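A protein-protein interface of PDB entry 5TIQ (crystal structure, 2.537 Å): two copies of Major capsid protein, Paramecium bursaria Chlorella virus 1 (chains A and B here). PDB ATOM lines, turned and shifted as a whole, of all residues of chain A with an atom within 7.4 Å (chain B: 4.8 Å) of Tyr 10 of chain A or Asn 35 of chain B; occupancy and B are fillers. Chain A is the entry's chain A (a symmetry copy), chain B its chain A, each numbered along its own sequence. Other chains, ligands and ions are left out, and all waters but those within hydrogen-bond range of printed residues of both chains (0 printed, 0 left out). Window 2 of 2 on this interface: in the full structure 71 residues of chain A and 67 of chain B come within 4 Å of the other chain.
Among the printed residues, pairs that only touch across the chains: Gln 6 of chain A with Ala 37 of chain B (3.8 Å), Leu 7 of chain A with Asn 35 of chain B (3.4 Å), Leu 7 of chain A with Phe 36 of chain B (3.6 Å), Leu 7 of chain A with Phe 209 of chain B (3.4 Å), Leu 7 of chain A with Leu 210 of chain B (3.5 Å), Tyr 10 of chain A with Asn 35 of chain B (3.4 Å), Thr 18 of chain A with Tyr 33 of chain B (3.2 Å), Thr 18 of chain A with Asn 35 of chain B (3.9 Å), Pro 21 of chain A with Tyr 33 of chain B (3.5 Å), Pro 21 of chain A with Thr 34 of chain B (3.5 Å), Ile 23 of chain A with Tyr 33 of chain B (3.3 Å) and Phe 26 of chain A with Phe 36 of chain B (3.6 Å).
O of Ile 23 of chain A sits at hydrogen-bond distance from N of Thr 34 of chain B (3.4 Å). O of Leu 17 of chain A sits at hydrogen-bond distance from N of Tyr 33 of chain B, at 3.2 Å.
Ala 9 of chain A touches none of the printed residues of chain B. Printed residues of chain B within 4 Å of Tyr 10 of chain A: Asn 35 (3.4 Å). Ala 12 of chain A touches none of the printed residues of chain B. Of the printed residues of chain A, Tyr 33 of chain B touches Leu 17, Thr 18, Pro 21 and Ile 23. Asn 35 of chain B touches just these residues of chain A: Leu 7, Tyr 10 and Thr 18. Of the printed residues of chain A, Leu 210 of chain B touches Leu 7 (3.5 Å). The nearest printed residue of chain B that does not touch Tyr 10 of chain A is Asp 211 of chain B (4.9 Å). The nearest residue of chain A that does not touch Asn 35 of chain B is Pro 21 of chain A (5.1 Å). The nearest printed residue of chain A that does not touch Leu 210 of chain B is Phe 26 of chain A (4.1 Å).
The backbone carbonyl oxygen of Ala 37 of chain B lies within hydrogen-bond range of the backbone NH of Phe 209 of chain B. The side-chain hydroxyl (OG1) of Thr 18 of chain A lies within hydrogen-bond range of the backbone carbonyl oxygen (O) of Asp 14 of chain A, at 3.1 Å.
Of the 19 printed residues of chain A, 8 touch a printed residue of chain B. Printed residues of chain A that touch a printed residue of chain B: Gln 6, Leu 7, Tyr 10, Leu 17, Thr 18, Pro 21, Ile 23 and Phe 26. Hydrophobic or aromatic side chains of chain A that line the printed part of chain B: Leu 7, Tyr 10, Pro 21, Ile 23 and Phe 26. Of the 8 printed residues of chain B, 7 touch a printed residue of chain A. Hydrophobic or aromatic side chains of chain B that line the printed part of chain A: Tyr 33, Phe 36, Ala 37 and Phe 209. Among the printed residues, no Asp or Glu carboxylate lies within 4 Å of a Lys or Arg side-chain nitrogen of the other chain.
No position is printed for both chains. Of the 14 pairs that touch across the chains among the printed residues, none has its exchanged pair printed and touching as well.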
ATOM      1  N   SER A   5      12.069 -17.781 -24.905  1.00  0.00           N
ATOM      2  CA  SER A   5      11.662 -18.518 -26.092  1.00  0.00           C
ATOM      3  C   SER A   5      10.166 -18.806 -26.108  1.00  0.00           C
ATOM      4  O   SER A   5       9.600 -19.003 -27.190  1.00  0.00           O
ATOM      5  CB  SER A   5      12.454 -19.826 -26.197  1.00  0.00           C
ATOM      6  OG  SER A   5      12.142 -20.709 -25.136  1.00  0.00           O
ATOM      7  N   GLN A   6       9.511 -18.830 -24.944  1.00  0.00           N
ATOM      8  CA  GLN A   6       8.064 -19.021 -24.910  1.00  0.00           C
ATOM      9  C   GLN A   6       7.311 -17.766 -25.336  1.00  0.00           C
ATOM     10  O   GLN A   6       6.257 -17.873 -25.970  1.00  0.00           O
ATOM     11  CB  GLN A   6       7.621 -19.454 -23.508  1.00  0.00           C
ATOM     12  CG  GLN A   6       6.123 -19.685 -23.369  1.00  0.00           C
ATOM     13  CD  GLN A   6       5.735 -20.150 -21.978  1.00  0.00           C
ATOM     14  OE1 GLN A   6       6.256 -21.149 -21.480  1.00  0.00           O
ATOM     15  NE2 GLN A   6       4.822 -19.423 -21.339  1.00  0.00           N
ATOM     16  N   LEU A   7       7.833 -16.580 -25.001  1.00  0.00           N
ATOM     17  CA  LEU A   7       7.208 -15.336 -25.441  1.00  0.00           C
ATOM     18  C   LEU A   7       7.128 -15.257 -26.959  1.00  0.00           C
ATOM     19  O   LEU A   7       6.150 -14.739 -27.512  1.00  0.00           O
ATOM     20  CB  LEU A   7       7.982 -14.135 -24.897  1.00  0.00           C
ATOM     21  CG  LEU A   7       7.668 -13.688 -23.473  1.00  0.00           C
ATOM     22  CD1 LEU A   7       8.565 -12.528 -23.076  1.00  0.00           C
ATOM     23  CD2 LEU A   7       6.209 -13.299 -23.372  1.00  0.00           C
ATOM     24  N   VAL A   8       8.152 -15.762 -27.651  1.00  0.00           N
ATOM     25  CA  VAL A   8       8.173 -15.690 -29.108  1.00  0.00           C
ATOM     26  C   VAL A   8       7.158 -16.651 -29.716  1.00  0.00           C
ATOM     27  O   VAL A   8       6.674 -16.429 -30.833  1.00  0.00           O
ATOM     28  CB  VAL A   8       9.598 -15.961 -29.628  1.00  0.00           C
ATOM     29  CG1 VAL A   8       9.694 -15.663 -31.120  1.00  0.00           C
ATOM     30  CG2 VAL A   8      10.610 -15.134 -28.846  1.00  0.00           C
ATOM     31  N   ALA A   9       6.809 -17.722 -29.002  1.00  0.00           N
ATOM     32  CA  ALA A   9       5.804 -18.663 -29.483  1.00  0.00           C
ATOM     33  C   ALA A   9       4.416 -18.038 -29.420  1.00  0.00           C
ATOM     34  O   ALA A   9       3.600 -18.400 -28.565  1.00  0.00           O
ATOM     35  CB  ALA A   9       5.848 -19.958 -28.669  1.00  0.00           C
ATOM     36  N   TYR A  10       4.143 -17.102 -30.325  1.00  0.00           N
ATOM     37  CA  TYR A  10       2.896 -16.351 -30.349  1.00  0.00           C
ATOM     38  C   TYR A  10       2.140 -16.667 -31.631  1.00  0.00           C
ATOM     39  O   TYR A  10       2.740 -16.766 -32.706  1.00  0.00           O
ATOM     40  CB  TYR A  10       3.170 -14.848 -30.247  1.00  0.00           C
ATOM     41  CG  TYR A  10       2.069 -14.053 -29.589  1.00  0.00           C
ATOM     42  CD1 TYR A  10       1.952 -14.009 -28.204  1.00  0.00           C
ATOM     43  CD2 TYR A  10       1.154 -13.332 -30.347  1.00  0.00           C
ATOM     44  CE1 TYR A  10       0.950 -13.277 -27.593  1.00  0.00           C
ATOM     45  CE2 TYR A  10       0.148 -12.598 -29.746  1.00  0.00           C
ATOM     46  CZ  TYR A  10       0.051 -12.572 -28.368  1.00  0.00           C
ATOM     47  OH  TYR A  10      -0.950 -11.844 -27.766  1.00  0.00           O
ATOM     48  N   GLY A  11       0.819 -16.826 -31.517  1.00  0.00           N
ATOM     49  CA  GLY A  11       0.000 -17.213 -32.647  1.00  0.00           C
ATOM     50  C   GLY A  11      -1.353 -16.527 -32.630  1.00  0.00           C
ATOM     51  O   GLY A  11      -1.648 -15.706 -31.760  1.00  0.00           O
ATOM     52  N   ALA A  12      -2.175 -16.891 -33.617  1.00  0.00           N
ATOM     53  CA  ALA A  12      -3.500 -16.296 -33.755  1.00  0.00           C
ATOM     54  C   ALA A  12      -4.402 -16.632 -32.573  1.00  0.00           C
ATOM     55  O   ALA A  12      -5.291 -15.844 -32.231  1.00  0.00           O
ATOM     56  CB  ALA A  12      -4.146 -16.755 -35.062  1.00  0.00           C
ATOM     57  N   GLN A  13      -4.206 -17.796 -31.950  1.00  0.00           N
ATOM     58  CA  GLN A  13      -5.040 -18.171 -30.813  1.00  0.00           C
ATOM     59  C   GLN A  13      -4.780 -17.303 -29.589  1.00  0.00           C
ATOM     60  O   GLN A  13      -5.637 -17.230 -28.702  1.00  0.00           O
ATOM     61  CB  GLN A  13      -4.825 -19.645 -30.464  1.00  0.00           C
ATOM     62  CG  GLN A  13      -5.098 -20.601 -31.614  1.00  0.00           C
ATOM     63  CD  GLN A  13      -4.823 -22.047 -31.251  1.00  0.00           C
ATOM     64  OE1 GLN A  13      -5.206 -22.509 -30.177  1.00  0.00           O
ATOM     65  NE2 GLN A  13      -4.156 -22.767 -32.144  1.00  0.00           N
ATOM     66  N   ASP A  14      -3.627 -16.634 -29.520  1.00  0.00           N
ATOM     67  CA  ASP A  14      -3.335 -15.766 -28.386  1.00  0.00           C
ATOM     68  C   ASP A  14      -4.104 -14.453 -28.429  1.00  0.00           C
ATOM     69  O   ASP A  14      -4.077 -13.712 -27.441  1.00  0.00           O
ATOM     70  CB  ASP A  14      -1.835 -15.477 -28.322  1.00  0.00           C
ATOM     71  CG  ASP A  14      -1.013 -16.721 -28.057  1.00  0.00           C
ATOM     72  OD1 ASP A  14      -1.346 -17.465 -27.108  1.00  0.00           O
ATOM     73  OD2 ASP A  14      -0.040 -16.959 -28.802  1.00  0.00           O
ATOM     74  N   VAL A  15      -4.784 -14.152 -29.538  1.00  0.00           N
ATOM     75  CA  VAL A  15      -5.516 -12.892 -29.653  1.00  0.00           C
ATOM     76  C   VAL A  15      -6.658 -12.838 -28.644  1.00  0.00           C
ATOM     77  O   VAL A  15      -6.955 -11.779 -28.076  1.00  0.00           O
ATOM     78  CB  VAL A  15      -6.014 -12.704 -31.097  1.00  0.00           C
ATOM     79  CG1 VAL A  15      -6.951 -11.528 -31.184  1.00  0.00           C
ATOM     80  CG2 VAL A  15      -4.835 -12.511 -32.043  1.00  0.00           C
ATOM     81  N   TYR A  16      -7.314 -13.974 -28.399  1.00  0.00           N
ATOM     82  CA  TYR A  16      -8.400 -14.006 -27.426  1.00  0.00           C
ATOM     83  C   TYR A  16      -7.907 -13.852 -25.996  1.00  0.00           C
ATOM     84  O   TYR A  16      -8.699 -13.498 -25.116  1.00  0.00           O
ATOM     85  CB  TYR A  16      -9.195 -15.308 -27.545  1.00  0.00           C
ATOM     86  CG  TYR A  16     -10.191 -15.336 -28.680  1.00  0.00           C
ATOM     87  CD1 TYR A  16     -11.478 -14.841 -28.503  1.00  0.00           C
ATOM     88  CD2 TYR A  16      -9.858 -15.869 -29.920  1.00  0.00           C
ATOM     89  CE1 TYR A  16     -12.403 -14.864 -29.527  1.00  0.00           C
ATOM     90  CE2 TYR A  16     -10.780 -15.897 -30.955  1.00  0.00           C
ATOM     91  CZ  TYR A  16     -12.053 -15.392 -30.751  1.00  0.00           C
ATOM     92  OH  TYR A  16     -12.982 -15.411 -31.769  1.00  0.00           O
ATOM     93  N   LEU A  17      -6.623 -14.102 -25.740  1.00  0.00           N
ATOM     94  CA  LEU A  17      -6.089 -14.077 -24.384  1.00  0.00           C
ATOM     95  C   LEU A  17      -5.299 -12.810 -24.083  1.00  0.00           C
ATOM     96  O   LEU A  17      -5.501 -12.191 -23.035  1.00  0.00           O
ATOM     97  CB  LEU A  17      -5.207 -15.309 -24.140  1.00  0.00           C
ATOM     98  CG  LEU A  17      -5.886 -16.675 -24.268  1.00  0.00           C
ATOM     99  CD1 LEU A  17      -4.990 -17.768 -23.709  1.00  0.00           C
ATOM    100  CD2 LEU A  17      -7.237 -16.677 -23.567  1.00  0.00           C
ATOM    101  N   THR A  18      -4.396 -12.414 -24.978  1.00  0.00           N
ATOM    102  CA  THR A  18      -3.486 -11.310 -24.713  1.00  0.00           C
ATOM    103  C   THR A  18      -3.513 -10.207 -25.763  1.00  0.00           C
ATOM    104  O   THR A  18      -2.742  -9.249 -25.643  1.00  0.00           O
ATOM    105  CB  THR A  18      -2.047 -11.832 -24.566  1.00  0.00           C
ATOM    106  OG1 THR A  18      -1.688 -12.592 -25.727  1.00  0.00           O
ATOM    107  CG2 THR A  18      -1.921 -12.707 -23.323  1.00  0.00           C
ATOM    108  N   GLY A  19      -4.359 -10.311 -26.786  1.00  0.00           N
ATOM    109  CA  GLY A  19      -4.421  -9.288 -27.813  1.00  0.00           C
ATOM    110  C   GLY A  19      -5.017  -8.003 -27.266  1.00  0.00           C
ATOM    111  O   GLY A  19      -6.144  -8.011 -26.743  1.00  0.00           O
ATOM    112  N   ASN A  20      -4.281  -6.890 -27.384  1.00  0.00           N
ATOM    113  CA  ASN A  20      -4.657  -5.598 -26.818  1.00  0.00           C
ATOM    114  C   ASN A  20      -4.999  -5.752 -25.342  1.00  0.00           C
ATOM    115  O   ASN A  20      -6.182  -5.806 -24.981  1.00  0.00           O
ATOM    116  CB  ASN A  20      -5.836  -4.979 -27.570  1.00  0.00           C
ATOM    117  CG  ASN A  20      -5.397  -4.171 -28.770  1.00  0.00           C
ATOM    118  OD1 ASN A  20      -5.805  -4.443 -29.896  1.00  0.00           O
ATOM    119  ND2 ASN A  20      -4.556  -3.169 -28.533  1.00  0.00           N
ATOM    120  N   PRO A  21      -3.997  -5.814 -24.467  1.00  0.00           N
ATOM    121  CA  PRO A  21      -4.269  -6.108 -23.056  1.00  0.00           C
ATOM    122  C   PRO A  21      -5.113  -5.023 -22.406  1.00  0.00           C
ATOM    123  O   PRO A  21      -4.991  -3.838 -22.722  1.00  0.00           O
ATOM    124  CB  PRO A  21      -2.870  -6.181 -22.432  1.00  0.00           C
ATOM    125  CG  PRO A  21      -1.941  -6.416 -23.582  1.00  0.00           C
ATOM    126  CD  PRO A  21      -2.556  -5.693 -24.738  1.00  0.00           C
ATOM    127  N   ILE A  23      -5.739  -5.559 -18.708  1.00  0.00           N
ATOM    128  CA  ILE A  23      -5.208  -5.610 -17.356  1.00  0.00           C
ATOM    129  C   ILE A  23      -3.782  -6.140 -17.410  1.00  0.00           C
ATOM    130  O   ILE A  23      -3.333  -6.692 -18.414  1.00  0.00           O
ATOM    131  CB  ILE A  23      -6.065  -6.490 -16.422  1.00  0.00           C
ATOM    132  CG1 ILE A  23      -5.907  -7.966 -16.798  1.00  0.00           C
ATOM    133  CG2 ILE A  23      -7.527  -6.071 -16.481  1.00  0.00           C
ATOM    134  CD1 ILE A  23      -6.514  -8.931 -15.791  1.00  0.00           C
ATOM    135  N   PHE A  26       0.938  -7.640 -12.923  1.00  0.00           N
ATOM    136  CA  PHE A  26       2.188  -7.290 -12.260  1.00  0.00           C
ATOM    137  C   PHE A  26       2.240  -5.823 -11.845  1.00  0.00           C
ATOM    138  O   PHE A  26       3.325  -5.301 -11.570  1.00  0.00           O
ATOM    139  CB  PHE A  26       3.371  -7.636 -13.166  1.00  0.00           C
ATOM    140  CG  PHE A  26       3.315  -9.031 -13.720  1.00  0.00           C
ATOM    141  CD1 PHE A  26       3.511 -10.126 -12.895  1.00  0.00           C
ATOM    142  CD2 PHE A  26       3.046  -9.247 -15.063  1.00  0.00           C
ATOM    143  CE1 PHE A  26       3.451 -11.413 -13.401  1.00  0.00           C
ATOM    144  CE2 PHE A  26       2.985 -10.532 -15.575  1.00  0.00           C
ATOM    145  CZ  PHE A  26       3.187 -11.616 -14.741  1.00  0.00           C
ATOM    146  N   TYR B  33      -4.968  -9.875 -20.862  1.00  0.00           N
ATOM    147  CA  TYR B  33      -3.829  -9.454 -20.061  1.00  0.00           C
ATOM    148  C   TYR B  33      -2.575  -9.359 -20.922  1.00  0.00           C
ATOM    149  O   TYR B  33      -2.558  -9.759 -22.088  1.00  0.00           O
ATOM    150  CB  TYR B  33      -3.600 -10.421 -18.895  1.00  0.00           C
ATOM    151  CG  TYR B  33      -3.420 -11.857 -19.329  1.00  0.00           C
ATOM    152  CD1 TYR B  33      -4.517 -12.685 -19.525  1.00  0.00           C
ATOM    153  CD2 TYR B  33      -2.155 -12.387 -19.539  1.00  0.00           C
ATOM    154  CE1 TYR B  33      -4.359 -13.999 -19.925  1.00  0.00           C
ATOM    155  CE2 TYR B  33      -1.987 -13.701 -19.937  1.00  0.00           C
ATOM    156  CZ  TYR B  33      -3.092 -14.500 -20.128  1.00  0.00           C
ATOM    157  OH  TYR B  33      -2.934 -15.808 -20.525  1.00  0.00           O
ATOM    158  N   THR B  34      -1.514  -8.817 -20.329  1.00  0.00           N
ATOM    159  CA  THR B  34      -0.240  -8.700 -21.024  1.00  0.00           C
ATOM    160  C   THR B  34       0.463 -10.049 -21.078  1.00  0.00           C
ATOM    161  O   THR B  34       0.502 -10.788 -20.090  1.00  0.00           O
ATOM    162  CB  THR B  34       0.660  -7.667 -20.342  1.00  0.00           C
ATOM    163  OG1 THR B  34       0.849  -8.023 -18.968  1.00  0.00           O
ATOM    164  CG2 THR B  34       0.047  -6.278 -20.421  1.00  0.00           C
ATOM    165  N   ASN B  35       1.016 -10.367 -22.245  1.00  0.00           N
ATOM    166  CA  ASN B  35       1.702 -11.634 -22.444  1.00  0.00           C
ATOM    167  C   ASN B  35       2.975 -11.696 -21.604  1.00  0.00           C
ATOM    168  O   ASN B  35       3.665 -10.688 -21.420  1.00  0.00           O
ATOM    169  CB  ASN B  35       2.036 -11.819 -23.923  1.00  0.00           C
ATOM    170  CG  ASN B  35       2.501 -13.221 -24.246  1.00  0.00           C
ATOM    171  OD1 ASN B  35       2.083 -14.188 -23.610  1.00  0.00           O
ATOM    172  ND2 ASN B  35       3.378 -13.338 -25.235  1.00  0.00           N
ATOM    173  N   PHE B  36       3.290 -12.885 -21.097  1.00  0.00           N
ATOM    174  CA  PHE B  36       4.454 -13.047 -20.234  1.00  0.00           C
ATOM    175  C   PHE B  36       4.818 -14.523 -20.156  1.00  0.00           C
ATOM    176  O   PHE B  36       4.099 -15.391 -20.655  1.00  0.00           O
ATOM    177  CB  PHE B  36       4.196 -12.482 -18.831  1.00  0.00           C
ATOM    178  CG  PHE B  36       3.234 -13.301 -18.020  1.00  0.00           C
ATOM    179  CD1 PHE B  36       1.866 -13.143 -18.175  1.00  0.00           C
ATOM    180  CD2 PHE B  36       3.698 -14.239 -17.111  1.00  0.00           C
ATOM    181  CE1 PHE B  36       0.979 -13.902 -17.435  1.00  0.00           C
ATOM    182  CE2 PHE B  36       2.815 -15.003 -16.372  1.00  0.00           C
ATOM    183  CZ  PHE B  36       1.455 -14.832 -16.533  1.00  0.00           C
ATOM    184  N   ALA B  37       5.944 -14.792 -19.498  1.00  0.00           N
ATOM    185  CA  ALA B  37       6.408 -16.148 -19.254  1.00  0.00           C
ATOM    186  C   ALA B  37       7.156 -16.175 -17.929  1.00  0.00           C
ATOM    187  O   ALA B  37       7.730 -15.168 -17.506  1.00  0.00           O
ATOM    188  CB  ALA B  37       7.311 -16.653 -20.386  1.00  0.00           C
ATOM    189  N   PHE B 209       9.208 -12.773 -17.700  1.00  0.00           N
ATOM    190  CA  PHE B 209       9.676 -12.213 -18.960  1.00  0.00           C
ATOM    191  C   PHE B 209       8.516 -11.480 -19.621  1.00  0.00           C
ATOM    192  O   PHE B 209       7.482 -12.088 -19.914  1.00  0.00           O
ATOM    193  CB  PHE B 209      10.221 -13.306 -19.880  1.00  0.00           C
ATOM    194  CG  PHE B 209      11.440 -14.000 -19.344  1.00  0.00           C
ATOM    195  CD1 PHE B 209      11.319 -15.066 -18.466  1.00  0.00           C
ATOM    196  CD2 PHE B 209      12.710 -13.589 -19.722  1.00  0.00           C
ATOM    197  CE1 PHE B 209      12.442 -15.706 -17.973  1.00  0.00           C
ATOM    198  CE2 PHE B 209      13.836 -14.223 -19.232  1.00  0.00           C
ATOM    199  CZ  PHE B 209      13.701 -15.283 -18.356  1.00  0.00           C
ATOM    200  N   LEU B 210       8.687 -10.181 -19.850  1.00  0.00           N
ATOM    201  CA  LEU B 210       7.617  -9.324 -20.337  1.00  0.00           C
ATOM    202  C   LEU B 210       7.749  -9.082 -21.834  1.00  0.00           C
ATOM    203  O   LEU B 210       8.843  -9.140 -22.401  1.00  0.00           O
ATOM    204  CB  LEU B 210       7.615  -7.983 -19.601  1.00  0.00           C
ATOM    205  CG  LEU B 210       7.372  -8.028 -18.092  1.00  0.00           C
ATOM    206  CD1 LEU B 210       7.592  -6.654 -17.483  1.00  0.00           C
ATOM    207  CD2 LEU B 210       5.971  -8.544 -17.788  1.00  0.00           C
ATOM    208  N   ASP B 211       6.615  -8.794 -22.467  1.00  0.00           N
ATOM    209  CA  ASP B 211       6.604  -8.438 -23.875  1.00  0.00           C
ATOM    210  C   ASP B 211       7.147  -7.022 -24.066  1.00  0.00           C
ATOM    211  O   ASP B 211       7.289  -6.249 -23.114  1.00  0.00           O
ATOM    212  CB  ASP B 211       5.192  -8.555 -24.445  1.00  0.00           C
ATOM    213  CG  ASP B 211       5.175  -9.148 -25.837  1.00  0.00           C
ATOM    214  OD1 ASP B 211       6.126  -8.892 -26.608  1.00  0.00           O
ATOM    215  OD2 ASP B 211       4.210  -9.873 -26.161  1.00  0.00           O
